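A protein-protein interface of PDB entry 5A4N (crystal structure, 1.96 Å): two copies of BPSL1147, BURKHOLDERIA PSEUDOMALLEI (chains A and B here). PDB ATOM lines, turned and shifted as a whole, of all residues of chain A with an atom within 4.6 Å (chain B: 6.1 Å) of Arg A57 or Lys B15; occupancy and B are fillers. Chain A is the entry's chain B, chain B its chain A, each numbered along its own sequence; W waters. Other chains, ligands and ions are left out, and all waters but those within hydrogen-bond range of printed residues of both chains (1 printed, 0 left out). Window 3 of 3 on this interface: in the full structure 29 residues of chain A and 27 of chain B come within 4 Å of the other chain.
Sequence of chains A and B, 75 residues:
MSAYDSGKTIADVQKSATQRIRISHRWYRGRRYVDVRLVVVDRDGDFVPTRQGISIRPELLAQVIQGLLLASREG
The backbone carbonyl oxygen (O) of Lys B15 is in hydrogen-bond range of the guanidinium group (NH1) of Arg A57, 2.9 Å away. The side-chain amino group (NZ) of Lys B15 sits at hydrogen-bond distance from the backbone carbonyl oxygen (O) of Ser A55, at 3.3 Å.
The guanidinium group (NE) of Arg A57 is in salt-bridge range of the side-chain carboxylate (OE2) of Glu A59, at 2.6 Å. N of Val B13 is in hydrogen-bond range of O of Ile B21 (2.8 Å). The backbone carbonyl oxygen (O) of Ser B16 sits at hydrogen-bond distance from the side-chain amide nitrogen (NE2) of Gln B14. The guanidinium group of Arg B20 is in hydrogen-bond range of the side-chain amide oxygen of Gln B14 (2.6 Å).
Leu A60 touches Val B13 (CB to CG1, 3.97 Å). Leu A60 touches Gln B14. CG of Lys B15 touches CD1 of Leu A60, 3.8 Å away.
Of chain A, only Ser A55 (3.3 Å), Arg A57 (2.9 Å) and Leu A60 (3.8 Å) come within 4 Å of Lys B15. Printed residues of chain A within 4 Å of Gln B14: Leu A60 (3.5 Å). Printed residues of chain B within 4 Å of Leu A60: Val B13 (3.97 Å), Gln B14 (3.5 Å) and Lys B15 (3.8 Å). Of the printed residues of chain A, Val B13 touches Leu A60 (3.97 Å).
Printed residues of chain A that touch a printed residue of chain B: Ser A55, Arg A57 and Leu A60. Printed residues of chain B that touch a printed residue of chain A: Val B13, Gln B14 and Lys B15. Hydrophobic or aromatic side chains of chain B that line the printed part of chain A: Val B13. Among the printed residues, no Asp or Glu carboxylate lies within 4 Å of a Lys or Arg side-chain nitrogen of the other chain.
No position is printed for both chains. Of the 5 pairs that touch across the chains among the printed residues, none has its exchanged pair printed and touching as well.
Water W1 lies within hydrogen-bond range of the backbone carbonyl oxygen of Gln B14 (2.7 Å), the guanidinium group of Arg A57 (2.7 Å) and the backbone carbonyl oxygen of Lys B15 (2.9 Å).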
ATOM      1  N   TYR A  33     -14.009  16.038  11.297  1.00  0.00           N
ATOM      2  CA  TYR A  33     -12.577  15.726  11.089  1.00  0.00           C
ATOM      3  C   TYR A  33     -11.876  15.899  12.425  1.00  0.00           C
ATOM      4  O   TYR A  33     -12.341  16.647  13.286  1.00  0.00           O
ATOM      5  CB  TYR A  33     -11.897  16.744  10.097  1.00  0.00           C
ATOM      6  CG  TYR A  33     -12.320  16.512   8.685  1.00  0.00           C
ATOM      7  CD1 TYR A  33     -11.694  15.549   7.905  1.00  0.00           C
ATOM      8  CD2 TYR A  33     -13.395  17.218   8.126  1.00  0.00           C
ATOM      9  CE1 TYR A  33     -12.123  15.273   6.602  1.00  0.00           C
ATOM     10  CE2 TYR A  33     -13.834  16.946   6.820  1.00  0.00           C
ATOM     11  CZ  TYR A  33     -13.194  15.980   6.066  1.00  0.00           C
ATOM     12  OH  TYR A  33     -13.602  15.704   4.784  1.00  0.00           O
ATOM     13  N   SER A  55      -5.553  17.462   8.871  1.00  0.00           N
ATOM     14  CA  SER A  55      -6.943  17.102   9.118  1.00  0.00           C
ATOM     15  C   SER A  55      -7.096  15.664   8.688  1.00  0.00           C
ATOM     16  O   SER A  55      -6.594  15.293   7.628  1.00  0.00           O
ATOM     17  CB  SER A  55      -7.857  17.938   8.263  1.00  0.00           C
ATOM     18  OG  SER A  55      -7.674  19.250   8.646  1.00  0.00           O
ATOM     19  N   ILE A  56      -7.792  14.883   9.507  1.00  0.00           N
ATOM     20  CA  ILE A  56      -7.811  13.430   9.475  1.00  0.00           C
ATOM     21  C   ILE A  56      -9.290  13.074   9.559  1.00  0.00           C
ATOM     22  O   ILE A  56      -9.908  13.396  10.552  1.00  0.00           O
ATOM     23  CB  ILE A  56      -7.116  12.865  10.759  1.00  0.00           C
ATOM     24  CG1 ILE A  56      -5.702  13.400  10.924  1.00  0.00           C
ATOM     25  CG2 ILE A  56      -7.053  11.387  10.760  1.00  0.00           C
ATOM     26  CD1 ILE A  56      -5.032  13.265  12.313  1.00  0.00           C
ATOM     27  N   ARG A  57      -9.867  12.415   8.561  1.00  0.00           N
ATOM     28  CA  ARG A  57     -11.215  11.893   8.773  1.00  0.00           C
ATOM     29  C   ARG A  57     -11.127  10.798   9.850  1.00  0.00           C
ATOM     30  O   ARG A  57     -10.098  10.171  10.001  1.00  0.00           O
ATOM     31  CB  ARG A  57     -11.926  11.410   7.480  1.00  0.00           C
ATOM     32  CG  ARG A  57     -11.269  10.288   6.724  1.00  0.00           C
ATOM     33  CD  ARG A  57     -12.139   9.826   5.561  1.00  0.00           C
ATOM     34  NE  ARG A  57     -11.550   8.685   4.863  1.00  0.00           N
ATOM     35  CZ  ARG A  57     -10.554   8.788   3.982  1.00  0.00           C
ATOM     36  NH1 ARG A  57     -10.049   9.963   3.659  1.00  0.00           N
ATOM     37  NH2 ARG A  57     -10.076   7.705   3.408  1.00  0.00           N
ATOM     38  N   PRO A  58     -12.213  10.609  10.629  1.00  0.00           N
ATOM     39  CA  PRO A  58     -12.141   9.705  11.771  1.00  0.00           C
ATOM     40  C   PRO A  58     -11.636   8.310  11.416  1.00  0.00           C
ATOM     41  O   PRO A  58     -10.900   7.747  12.188  1.00  0.00           O
ATOM     42  CB  PRO A  58     -13.591   9.703  12.293  1.00  0.00           C
ATOM     43  CG  PRO A  58     -14.083  11.033  11.917  1.00  0.00           C
ATOM     44  CD  PRO A  58     -13.517  11.298  10.582  1.00  0.00           C
ATOM     45  N   GLU A  59     -11.934   7.807  10.220  1.00  0.00           N
ATOM     46  CA  GLU A  59     -11.509   6.454   9.862  1.00  0.00           C
ATOM     47  C   GLU A  59      -9.994   6.363   9.654  1.00  0.00           C
ATOM     48  O   GLU A  59      -9.491   5.262   9.551  1.00  0.00           O
ATOM     49  CB  GLU A  59     -12.259   5.892   8.616  1.00  0.00           C
ATOM     50  CG  GLU A  59     -11.874   6.499   7.261  1.00  0.00           C
ATOM     51  CD  GLU A  59     -12.562   5.858   6.047  1.00  0.00           C
ATOM     52  OE1 GLU A  59     -13.482   5.035   6.222  1.00  0.00           O
ATOM     53  OE2 GLU A  59     -12.185   6.191   4.895  1.00  0.00           O
ATOM     54  N   LEU A  60      -9.263   7.481   9.612  1.00  0.00           N
ATOM     55  CA  LEU A  60      -7.790   7.391   9.470  1.00  0.00           C
ATOM     56  C   LEU A  60      -7.105   7.573  10.771  1.00  0.00           C
ATOM     57  O   LEU A  60      -5.888   7.423  10.854  1.00  0.00           O
ATOM     58  CB  LEU A  60      -7.285   8.407   8.472  1.00  0.00           C
ATOM     59  CG  LEU A  60      -7.891   8.278   7.088  1.00  0.00           C
ATOM     60  CD1 LEU A  60      -7.377   9.436   6.269  1.00  0.00           C
ATOM     61  CD2 LEU A  60      -7.571   6.937   6.424  1.00  0.00           C
ATOM     62  N   LEU A  61      -7.857   7.837  11.830  1.00  0.00           N
ATOM     63  CA  LEU A  61      -7.247   8.222  13.079  1.00  0.00           C
ATOM     64  C   LEU A  61      -6.447   7.060  13.683  1.00  0.00           C
ATOM     65  O   LEU A  61      -5.324   7.260  14.128  1.00  0.00           O
ATOM     66  CB  LEU A  61      -8.316   8.747  14.014  1.00  0.00           C
ATOM     67  CG  LEU A  61      -7.952   9.324  15.352  1.00  0.00           C
ATOM     68  CD1 LEU A  61      -6.986  10.461  15.141  1.00  0.00           C
ATOM     69  CD2 LEU A  61      -9.196   9.785  16.092  1.00  0.00           C
ATOM     70  N   VAL B  13      -0.204   7.169   5.598  1.00  0.00           N
ATOM     71  CA  VAL B  13      -1.641   6.937   5.734  1.00  0.00           C
ATOM     72  C   VAL B  13      -2.344   7.533   4.510  1.00  0.00           C
ATOM     73  O   VAL B  13      -2.339   8.746   4.328  1.00  0.00           O
ATOM     74  CB  VAL B  13      -2.150   7.619   6.994  1.00  0.00           C
ATOM     75  CG1 VAL B  13      -3.671   7.450   7.146  1.00  0.00           C
ATOM     76  CG2 VAL B  13      -1.363   7.121   8.210  1.00  0.00           C
ATOM     77  N   GLN B  14      -2.904   6.670   3.670  1.00  0.00           N
ATOM     78  CA  GLN B  14      -3.564   7.071   2.418  1.00  0.00           C
ATOM     79  C   GLN B  14      -4.870   7.763   2.761  1.00  0.00           C
ATOM     80  O   GLN B  14      -5.754   7.189   3.389  1.00  0.00           O
ATOM     81  CB  GLN B  14      -3.830   5.848   1.512  1.00  0.00           C
ATOM     82  CG  GLN B  14      -4.064   6.139   0.009  1.00  0.00           C
ATOM     83  CD  GLN B  14      -2.764   6.476  -0.742  1.00  0.00           C
ATOM     84  OE1 GLN B  14      -1.682   5.996  -0.377  1.00  0.00           O
ATOM     85  NE2 GLN B  14      -2.858   7.307  -1.789  1.00  0.00           N
ATOM     86  N   LYS B  15      -4.984   9.003   2.347  1.00  0.00           N
ATOM     87  CA  LYS B  15      -6.186   9.791   2.497  1.00  0.00           C
ATOM     88  C   LYS B  15      -7.082   9.590   1.283  1.00  0.00           C
ATOM     89  O   LYS B  15      -8.290   9.422   1.382  1.00  0.00           O
ATOM     90  CB  LYS B  15      -5.773  11.252   2.513  1.00  0.00           C
ATOM     91  CG  LYS B  15      -6.258  12.039   3.678  1.00  0.00           C
ATOM     92  CD  LYS B  15      -5.404  13.282   3.875  1.00  0.00           C
ATOM     93  CE  LYS B  15      -6.104  14.498   3.338  1.00  0.00           C
ATOM     94  NZ  LYS B  15      -7.102  14.875   4.348  1.00  0.00           N
ATOM     95  N   SER B  16      -6.459   9.622   0.116  1.00  0.00           N
ATOM     96  CA  SER B  16      -7.158   9.475  -1.136  1.00  0.00           C
ATOM     97  C   SER B  16      -6.135   9.069  -2.166  1.00  0.00           C
ATOM     98  O   SER B  16      -4.954   8.883  -1.849  1.00  0.00           O
ATOM     99  CB  SER B  16      -7.759  10.815  -1.553  1.00  0.00           C
ATOM    100  OG  SER B  16      -6.734  11.712  -1.948  1.00  0.00           O
ATOM    101  N   ALA B  17      -6.570   9.001  -3.414  1.00  0.00           N
ATOM    102  CA  ALA B  17      -5.697   8.623  -4.516  1.00  0.00           C
ATOM    103  C   ALA B  17      -4.555   9.604  -4.684  1.00  0.00           C
ATOM    104  O   ALA B  17      -3.455   9.225  -5.082  1.00  0.00           O
ATOM    105  CB  ALA B  17      -6.508   8.531  -5.815  1.00  0.00           C
ATOM    106  N   GLN B  19      -3.537  11.953  -2.135  1.00  0.00           N
ATOM    107  CA  GLN B  19      -3.049  12.547  -0.889  1.00  0.00           C
ATOM    108  C   GLN B  19      -2.753  11.517   0.191  1.00  0.00           C
ATOM    109  O   GLN B  19      -3.453  10.513   0.312  1.00  0.00           O
ATOM    110  CB  GLN B  19      -4.068  13.527  -0.316  1.00  0.00           C
ATOM    111  CG  GLN B  19      -4.454  14.686  -1.216  1.00  0.00           C
ATOM    112  CD  GLN B  19      -5.221  15.746  -0.440  1.00  0.00           C
ATOM    113  OE1 GLN B  19      -5.960  15.451   0.495  1.00  0.00           O
ATOM    114  NE2 GLN B  19      -5.030  16.986  -0.809  1.00  0.00           N
ATOM    115  N   ARG B  20      -1.716  11.787   0.980  1.00  0.00           N
ATOM    116  CA  ARG B  20      -1.362  10.930   2.118  1.00  0.00           C
ATOM    117  C   ARG B  20      -0.906  11.764   3.285  1.00  0.00           C
ATOM    118  O   ARG B  20      -0.384  12.870   3.110  1.00  0.00           O
ATOM    119  CB  ARG B  20      -0.199  10.022   1.774  1.00  0.00           C
ATOM    120  CG  ARG B  20      -0.417   9.191   0.567  1.00  0.00           C
ATOM    121  CD  ARG B  20       0.851   8.479   0.259  1.00  0.00           C
ATOM    122  NE  ARG B  20       0.571   7.300  -0.522  1.00  0.00           N
ATOM    123  CZ  ARG B  20       1.495   6.662  -1.229  1.00  0.00           C
ATOM    124  NH1 ARG B  20       2.763   7.085  -1.245  1.00  0.00           N
ATOM    125  NH2 ARG B  20       1.148   5.590  -1.928  1.00  0.00           N
ATOM    126  N   ILE B  21      -1.048  11.213   4.481  1.00  0.00           N
ATOM    127  CA  ILE B  21      -0.399  11.787   5.625  1.00  0.00           C
ATOM    128  C   ILE B  21       0.814  10.947   5.865  1.00  0.00           C
ATOM    129  O   ILE B  21       0.703   9.755   6.087  1.00  0.00           O
ATOM    130  CB  ILE B  21      -1.305  11.766   6.841  1.00  0.00           C
ATOM    131  CG1 ILE B  21      -2.532  12.597   6.522  1.00  0.00           C
ATOM    132  CG2 ILE B  21      -0.591  12.359   8.045  1.00  0.00           C
ATOM    133  CD1 ILE B  21      -3.722  12.191   7.359  1.00  0.00           C
ATOM    134  N   LEU B  38       1.042  16.379   5.306  1.00  0.00           N
ATOM    135  CA  LEU B  38       0.313  16.108   4.068  1.00  0.00           C
ATOM    136  C   LEU B  38       1.251  16.066   2.841  1.00  0.00           C
ATOM    137  O   LEU B  38       2.016  17.012   2.578  1.00  0.00           O
ATOM    138  CB  LEU B  38      -0.768  17.161   3.893  1.00  0.00           C
ATOM    139  CG  LEU B  38      -1.694  17.044   2.684  1.00  0.00           C
ATOM    140  CD1 LEU B  38      -2.604  15.833   2.826  1.00  0.00           C
ATOM    141  CD2 LEU B  38      -2.498  18.332   2.559  1.00  0.00           C
HETATM  142  O   HOH W   1      -7.993   6.569   2.032  1.00  0.00           O
